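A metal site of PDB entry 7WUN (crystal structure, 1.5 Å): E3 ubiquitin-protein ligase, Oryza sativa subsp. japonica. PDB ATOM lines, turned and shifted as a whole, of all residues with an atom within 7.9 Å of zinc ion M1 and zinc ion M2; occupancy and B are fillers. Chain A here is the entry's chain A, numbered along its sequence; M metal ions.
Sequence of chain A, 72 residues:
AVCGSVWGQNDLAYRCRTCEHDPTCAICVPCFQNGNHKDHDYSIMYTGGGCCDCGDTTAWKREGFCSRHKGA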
ATOM      1  N   ALA A   1      -2.798  13.691  -1.236  1.00  0.00           N
ATOM      2  CA  ALA A   1      -3.272  14.832  -2.011  1.00  0.00           C
ATOM      3  C   ALA A   1      -2.967  16.157  -1.312  1.00  0.00           C
ATOM      4  O   ALA A   1      -2.445  17.096  -1.923  1.00  0.00           O
ATOM      5  CB  ALA A   1      -4.767  14.714  -2.266  1.00  0.00           C
ATOM      6  N   VAL A   2      -3.323  16.220  -0.029  1.00  0.00           N
ATOM      7  CA  VAL A   2      -3.043  17.352   0.837  1.00  0.00           C
ATOM      8  C   VAL A   2      -2.202  16.845   2.000  1.00  0.00           C
ATOM      9  O   VAL A   2      -2.574  15.866   2.656  1.00  0.00           O
ATOM     10  CB  VAL A   2      -4.348  17.996   1.349  1.00  0.00           C
ATOM     11  CG1 VAL A   2      -4.049  18.993   2.479  1.00  0.00           C
ATOM     12  CG2 VAL A   2      -5.076  18.666   0.211  1.00  0.00           C
ATOM     13  N   CYS A   3      -1.086  17.518   2.256  1.00  0.00           N
ATOM     14  CA  CYS A   3      -0.152  17.076   3.286  1.00  0.00           C
ATOM     15  C   CYS A   3      -0.851  16.915   4.630  1.00  0.00           C
ATOM     16  O   CYS A   3      -1.472  17.850   5.138  1.00  0.00           O
ATOM     17  CB  CYS A   3       0.985  18.091   3.421  1.00  0.00           C
ATOM     18  SG  CYS A   3       2.235  17.628   4.649  1.00  0.00           S
ATOM     19  N   GLY A   4      -0.732  15.733   5.221  1.00  0.00           N
ATOM     20  CA  GLY A   4      -1.402  15.531   6.495  1.00  0.00           C
ATOM     21  C   GLY A   4      -0.576  15.891   7.716  1.00  0.00           C
ATOM     22  O   GLY A   4      -0.889  15.426   8.822  1.00  0.00           O
ATOM     23  N   SER A   5       0.461  16.710   7.573  1.00  0.00           N
ATOM     24  CA  SER A   5       1.383  16.893   8.682  1.00  0.00           C
ATOM     25  C   SER A   5       0.802  17.842   9.717  1.00  0.00           C
ATOM     26  O   SER A   5       0.194  18.865   9.380  1.00  0.00           O
ATOM     27  CB  SER A   5       2.742  17.388   8.201  1.00  0.00           C
ATOM     28  OG  SER A   5       3.737  17.085   9.173  1.00  0.00           O
ATOM     29  N   VAL A   6       0.974  17.480  10.967  1.00  0.00           N
ATOM     30  CA  VAL A   6       0.558  18.311  12.084  1.00  0.00           C
ATOM     31  C   VAL A   6       1.779  18.672  12.891  1.00  0.00           C
ATOM     32  O   VAL A   6       2.755  17.909  12.966  1.00  0.00           O
ATOM     33  CB  VAL A   6      -0.507  17.621  12.962  1.00  0.00           C
ATOM     34  CG1 VAL A   6      -1.652  17.141  12.103  1.00  0.00           C
ATOM     35  CG2 VAL A   6       0.120  16.441  13.675  1.00  0.00           C
ATOM     36  N   TRP A   7       1.753  19.854  13.483  1.00  0.00           N
ATOM     37  CA  TRP A   7       2.845  20.267  14.361  1.00  0.00           C
ATOM     38  C   TRP A   7       2.280  20.988  15.573  1.00  0.00           C
ATOM     39  O   TRP A   7       1.114  21.381  15.597  1.00  0.00           O
ATOM     40  CB  TRP A   7       3.882  21.133  13.623  1.00  0.00           C
ATOM     41  CG  TRP A   7       3.366  22.422  13.149  1.00  0.00           C
ATOM     42  CD1 TRP A   7       3.384  23.620  13.833  1.00  0.00           C
ATOM     43  CD2 TRP A   7       2.791  22.696  11.864  1.00  0.00           C
ATOM     44  NE1 TRP A   7       2.828  24.609  13.053  1.00  0.00           N
ATOM     45  CE2 TRP A   7       2.461  24.067  11.848  1.00  0.00           C
ATOM     46  CE3 TRP A   7       2.515  21.912  10.738  1.00  0.00           C
ATOM     47  CZ2 TRP A   7       1.860  24.674  10.738  1.00  0.00           C
ATOM     48  CZ3 TRP A   7       1.922  22.527   9.641  1.00  0.00           C
ATOM     49  CH2 TRP A   7       1.611  23.892   9.656  1.00  0.00           C
ATOM     50  N   ALA A  26      -0.485  28.017   6.526  1.00  0.00           N
ATOM     51  CA  ALA A  26       0.895  27.646   6.805  1.00  0.00           C
ATOM     52  C   ALA A  26       1.204  26.298   6.177  1.00  0.00           C
ATOM     53  O   ALA A  26       0.309  25.467   5.999  1.00  0.00           O
ATOM     54  CB  ALA A  26       1.178  27.593   8.312  1.00  0.00           C
ATOM     55  N   ILE A  27       2.486  26.081   5.874  1.00  0.00           N
ATOM     56  CA  ILE A  27       2.953  24.763   5.427  1.00  0.00           C
ATOM     57  C   ILE A  27       4.119  24.300   6.283  1.00  0.00           C
ATOM     58  O   ILE A  27       4.868  25.101   6.862  1.00  0.00           O
ATOM     59  CB  ILE A  27       3.328  24.738   3.929  1.00  0.00           C
ATOM     60  CG1 ILE A  27       4.520  25.645   3.610  1.00  0.00           C
ATOM     61  CG2 ILE A  27       2.119  25.090   3.059  1.00  0.00           C
ATOM     62  CD1 ILE A  27       4.954  25.505   2.151  1.00  0.00           C
ATOM     63  N   CYS A  28       4.250  22.982   6.395  1.00  0.00           N
ATOM     64  CA  CYS A  28       5.314  22.416   7.201  1.00  0.00           C
ATOM     65  C   CYS A  28       6.674  22.680   6.575  1.00  0.00           C
ATOM     66  O   CYS A  28       6.805  23.006   5.389  1.00  0.00           O
ATOM     67  CB  CYS A  28       5.075  20.903   7.380  1.00  0.00           C
ATOM     68  SG  CYS A  28       5.311  19.861   5.899  1.00  0.00           S
ATOM     69  N   VAL A  29       7.723  22.540   7.396  1.00  0.00           N
ATOM     70  CA  VAL A  29       9.071  22.828   6.914  1.00  0.00           C
ATOM     71  C   VAL A  29       9.437  21.961   5.705  1.00  0.00           C
ATOM     72  O   VAL A  29       9.924  22.505   4.704  1.00  0.00           O
ATOM     73  CB  VAL A  29      10.089  22.695   8.060  1.00  0.00           C
ATOM     74  CG1 VAL A  29      11.505  22.656   7.517  1.00  0.00           C
ATOM     75  CG2 VAL A  29       9.902  23.831   9.048  1.00  0.00           C
ATOM     76  N   PRO A  30       9.218  20.644   5.704  1.00  0.00           N
ATOM     77  CA  PRO A  30       9.570  19.876   4.498  1.00  0.00           C
ATOM     78  C   PRO A  30       8.805  20.286   3.248  1.00  0.00           C
ATOM     79  O   PRO A  30       9.382  20.285   2.157  1.00  0.00           O
ATOM     80  CB  PRO A  30       9.297  18.426   4.896  1.00  0.00           C
ATOM     81  CG  PRO A  30       9.188  18.406   6.356  1.00  0.00           C
ATOM     82  CD  PRO A  30       8.870  19.779   6.846  1.00  0.00           C
ATOM     83  N   CYS A  31       7.517  20.633   3.380  1.00  0.00           N
ATOM     84  CA  CYS A  31       6.791  21.103   2.192  1.00  0.00           C
ATOM     85  C   CYS A  31       7.356  22.417   1.682  1.00  0.00           C
ATOM     86  O   CYS A  31       7.419  22.639   0.471  1.00  0.00           O
ATOM     87  CB  CYS A  31       5.304  21.240   2.508  1.00  0.00           C
ATOM     88  SG  CYS A  31       4.497  19.653   2.517  1.00  0.00           S
ATOM     89  N   PHE A  32       7.779  23.301   2.584  1.00  0.00           N
ATOM     90  CA  PHE A  32       8.412  24.529   2.113  1.00  0.00           C
ATOM     91  C   PHE A  32       9.704  24.218   1.368  1.00  0.00           C
ATOM     92  O   PHE A  32       9.950  24.736   0.271  1.00  0.00           O
ATOM     93  CB  PHE A  32       8.707  25.464   3.282  1.00  0.00           C
ATOM     94  CG  PHE A  32       9.305  26.766   2.842  1.00  0.00           C
ATOM     95  CD1 PHE A  32       8.500  27.792   2.358  1.00  0.00           C
ATOM     96  CD2 PHE A  32      10.677  26.917   2.812  1.00  0.00           C
ATOM     97  CE1 PHE A  32       9.056  28.993   1.912  1.00  0.00           C
ATOM     98  CE2 PHE A  32      11.239  28.126   2.358  1.00  0.00           C
ATOM     99  CZ  PHE A  32      10.437  29.140   1.909  1.00  0.00           C
ATOM    100  N   ASN A  34      10.659  21.582  -0.181  1.00  0.00           N
ATOM    101  CA  ASN A  34      10.472  20.908  -1.447  1.00  0.00           C
ATOM    102  C   ASN A  34       9.588  21.680  -2.422  1.00  0.00           C
ATOM    103  O   ASN A  34       9.138  21.121  -3.431  1.00  0.00           O
ATOM    104  CB  ASN A  34       9.911  19.511  -1.208  1.00  0.00           C
ATOM    105  CG  ASN A  34      10.948  18.576  -0.640  1.00  0.00           C
ATOM    106  OD1 ASN A  34      12.136  18.715  -0.929  1.00  0.00           O
ATOM    107  ND2 ASN A  34      10.519  17.636   0.173  1.00  0.00           N
ATOM    108  N   GLY A  35       9.337  22.970  -2.166  1.00  0.00           N
ATOM    109  CA  GLY A  35       8.612  23.826  -3.075  1.00  0.00           C
ATOM    110  C   GLY A  35       9.461  25.004  -3.527  1.00  0.00           C
ATOM    111  O   GLY A  35      10.645  25.119  -3.194  1.00  0.00           O
ATOM    112  N   CYS A  51      -1.843  22.455  11.025  1.00  0.00           N
ATOM    113  CA  CYS A  51      -1.928  21.376  10.048  1.00  0.00           C
ATOM    114  C   CYS A  51      -1.496  21.930   8.697  1.00  0.00           C
ATOM    115  O   CYS A  51      -1.889  23.041   8.328  1.00  0.00           O
ATOM    116  CB  CYS A  51      -3.332  20.827   9.908  1.00  0.00           C
ATOM    117  SG  CYS A  51      -4.017  20.060  11.356  1.00  0.00           S
ATOM    118  N   CYS A  52      -0.718  21.145   7.952  1.00  0.00           N
ATOM    119  CA  CYS A  52      -0.133  21.670   6.722  1.00  0.00           C
ATOM    120  C   CYS A  52      -1.196  21.912   5.653  1.00  0.00           C
ATOM    121  O   CYS A  52      -2.105  21.086   5.458  1.00  0.00           O
ATOM    122  CB  CYS A  52       0.929  20.716   6.214  1.00  0.00           C
ATOM    123  SG  CYS A  52       1.832  21.337   4.809  1.00  0.00           S
ATOM    124  N   ASP A  53      -1.073  23.036   4.941  1.00  0.00           N
ATOM    125  CA  ASP A  53      -2.001  23.371   3.872  1.00  0.00           C
ATOM    126  C   ASP A  53      -1.494  22.996   2.484  1.00  0.00           C
ATOM    127  O   ASP A  53      -2.182  23.262   1.491  1.00  0.00           O
ATOM    128  CB  ASP A  53      -2.298  24.878   3.908  1.00  0.00           C
ATOM    129  CG  ASP A  53      -3.082  25.282   5.144  1.00  0.00           C
ATOM    130  OD1 ASP A  53      -3.957  24.502   5.590  1.00  0.00           O
ATOM    131  OD2 ASP A  53      -2.796  26.362   5.682  1.00  0.00           O
ATOM    132  N   CYS A  54      -0.322  22.360   2.395  1.00  0.00           N
ATOM    133  CA  CYS A  54       0.267  22.073   1.095  1.00  0.00           C
ATOM    134  C   CYS A  54      -0.588  21.066   0.346  1.00  0.00           C
ATOM    135  O   CYS A  54      -0.885  19.980   0.862  1.00  0.00           O
ATOM    136  CB  CYS A  54       1.689  21.553   1.247  1.00  0.00           C
ATOM    137  SG  CYS A  54       2.500  21.227  -0.293  1.00  0.00           S
ATOM    138  N   GLY A  55      -0.967  21.422  -0.879  1.00  0.00           N
ATOM    139  CA  GLY A  55      -1.840  20.621  -1.716  1.00  0.00           C
ATOM    140  C   GLY A  55      -3.298  21.047  -1.708  1.00  0.00           C
ATOM    141  O   GLY A  55      -4.059  20.588  -2.563  1.00  0.00           O
ATOM    142  N   GLY A  64       2.601  27.227  -5.216  1.00  0.00           N
ATOM    143  CA  GLY A  64       3.288  27.043  -3.961  1.00  0.00           C
ATOM    144  C   GLY A  64       3.245  25.641  -3.376  1.00  0.00           C
ATOM    145  O   GLY A  64       3.770  25.449  -2.274  1.00  0.00           O
ATOM    146  N   PHE A  65       2.656  24.673  -4.074  1.00  0.00           N
ATOM    147  CA  PHE A  65       2.680  23.282  -3.627  1.00  0.00           C
ATOM    148  C   PHE A  65       4.076  22.710  -3.784  1.00  0.00           C
ATOM    149  O   PHE A  65       4.785  22.992  -4.758  1.00  0.00           O
ATOM    150  CB  PHE A  65       1.715  22.427  -4.452  1.00  0.00           C
ATOM    151  CG  PHE A  65       0.261  22.776  -4.280  1.00  0.00           C
ATOM    152  CD1 PHE A  65      -0.174  23.647  -3.295  1.00  0.00           C
ATOM    153  CD2 PHE A  65      -0.690  22.180  -5.098  1.00  0.00           C
ATOM    154  CE1 PHE A  65      -1.521  23.940  -3.148  1.00  0.00           C
ATOM    155  CE2 PHE A  65      -2.048  22.455  -4.964  1.00  0.00           C
ATOM    156  CZ  PHE A  65      -2.464  23.341  -3.985  1.00  0.00           C
ATOM    157  N   CYS A  66       4.477  21.875  -2.827  1.00  0.00           N
ATOM    158  CA  CYS A  66       5.749  21.197  -2.989  1.00  0.00           C
ATOM    159  C   CYS A  66       5.619  20.112  -4.049  1.00  0.00           C
ATOM    160  O   CYS A  66       4.534  19.831  -4.571  1.00  0.00           O
ATOM    161  CB  CYS A  66       6.231  20.616  -1.648  1.00  0.00           C
ATOM    162  SG  CYS A  66       5.529  19.011  -1.202  1.00  0.00           S
ATOM    163  N   SER A  67       6.755  19.501  -4.396  1.00  0.00           N
ATOM    164  CA  SER A  67       6.774  18.494  -5.448  1.00  0.00           C
ATOM    165  C   SER A  67       5.963  17.251  -5.103  1.00  0.00           C
ATOM    166  O   SER A  67       5.591  16.508  -6.012  1.00  0.00           O
ATOM    167  CB  SER A  67       8.211  18.099  -5.741  1.00  0.00           C
ATOM    168  OG  SER A  67       8.852  17.709  -4.534  1.00  0.00           O
ATOM    169  N   ARG A  68       5.680  17.017  -3.818  1.00  0.00           N
ATOM    170  CA  ARG A  68       5.067  15.772  -3.380  1.00  0.00           C
ATOM    171  C   ARG A  68       3.566  15.884  -3.153  1.00  0.00           C
ATOM    172  O   ARG A  68       2.900  14.848  -3.025  1.00  0.00           O
ATOM    173  CB  ARG A  68       5.751  15.284  -2.088  1.00  0.00           C
ATOM    174  CG  ARG A  68       7.203  14.936  -2.304  1.00  0.00           C
ATOM    175  CD  ARG A  68       7.908  14.430  -1.045  1.00  0.00           C
ATOM    176  NE  ARG A  68       7.283  13.231  -0.520  1.00  0.00           N
ATOM    177  CZ  ARG A  68       6.451  13.210   0.512  1.00  0.00           C
ATOM    178  NH1 ARG A  68       6.193  14.299   1.215  1.00  0.00           N
ATOM    179  NH2 ARG A  68       5.873  12.060   0.865  1.00  0.00           N
ATOM    180  N   HIS A  69       3.027  17.081  -3.114  1.00  0.00           N
ATOM    181  CA  HIS A  69       1.585  17.290  -3.071  1.00  0.00           C
ATOM    182  C   HIS A  69       1.182  18.222  -4.205  1.00  0.00           C
ATOM    183  O   HIS A  69       0.349  19.115  -4.042  1.00  0.00           O
ATOM    184  CB  HIS A  69       1.168  17.825  -1.688  1.00  0.00           C
ATOM    185  CG  HIS A  69       1.770  17.070  -0.538  1.00  0.00           C
ATOM    186  ND1 HIS A  69       2.823  17.560   0.206  1.00  0.00           N
ATOM    187  CD2 HIS A  69       1.479  15.856  -0.025  1.00  0.00           C
ATOM    188  CE1 HIS A  69       3.149  16.676   1.139  1.00  0.00           C
ATOM    189  NE2 HIS A  69       2.350  15.624   1.018  1.00  0.00           N
ATOM    190  N   LYS A  70       1.815  18.046  -5.370  1.00  0.00           N
ATOM    191  CA  LYS A  70       1.485  18.797  -6.593  1.00  0.00           C
ATOM    192  C   LYS A  70       0.609  17.955  -7.502  1.00  0.00           C
ATOM    193  O   LYS A  70      -0.315  17.296  -7.038  1.00  0.00           O
ATOM    194  CB  LYS A  70       2.746  19.232  -7.358  1.00  0.00           C
ATOM    195  CG  LYS A  70       3.157  20.684  -7.100  1.00  0.00           C
ATOM    196  CD  LYS A  70       3.771  21.377  -8.295  1.00  0.00           C
ATOM    197  CE  LYS A  70       2.822  22.441  -8.865  1.00  0.00           C
ATOM    198  NZ  LYS A  70       3.469  23.270  -9.934  1.00  0.00           N
HETATM  199 ZN    ZN M   1       3.772  19.385   0.258  1.00  0.00          ZN
HETATM  200 ZN    ZN M   2       3.372  19.613   4.607  1.00  0.00          ZN
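Zinc ion M2 is bound by SG of Cys 3 (2.3 Å). Zinc ion M2 is bound by the side-chain sulfur (SG) of Cys 52. SG of Cys 28 is bound to zinc ion M2 (2.3 Å). SG of Cys 31 binds zinc ion M2, 2.4 Å away. Zinc ion M2 has four donor atoms within binding distance.
Zinc ion M1 is bound by a ring nitrogen (ND1) of His 69 (2.1 Å), the side-chain sulfur (SG) of Cys 54 (2.3 Å), the side-chain sulfur (SG) of Cys 66 (2.3 Å) and the side-chain sulfur (SG) of Cys 31 (2.4 Å). Zinc ion M1 has four donor atoms within binding distance.
The backbone carbonyl oxygen (O) of Cys 54 is in hydrogen-bond range of the backbone NH (N) of Cys 3 (2.8 Å). The side-chain sulfur (SG) of Cys 3 lies close to the backbone NH (N) of Ser 5 (3.5 Å). N of Cys 54 sits close to SG of Cys 52, at 3.4 Å. The side-chain sulfur (SG) of Cys 66 sits close to the backbone NH (N) of Arg 68, at 3.3 Å. N of Cys 52 is in hydrogen-bond range of O of Ser 5 (2.8 Å).
Within 4 Å of zinc ion M1: Cys 31, Cys 54, Cys 66 and His 69. The nearest printed residue that does not touch zinc ion M1 is Cys 3 (4.4 Å).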
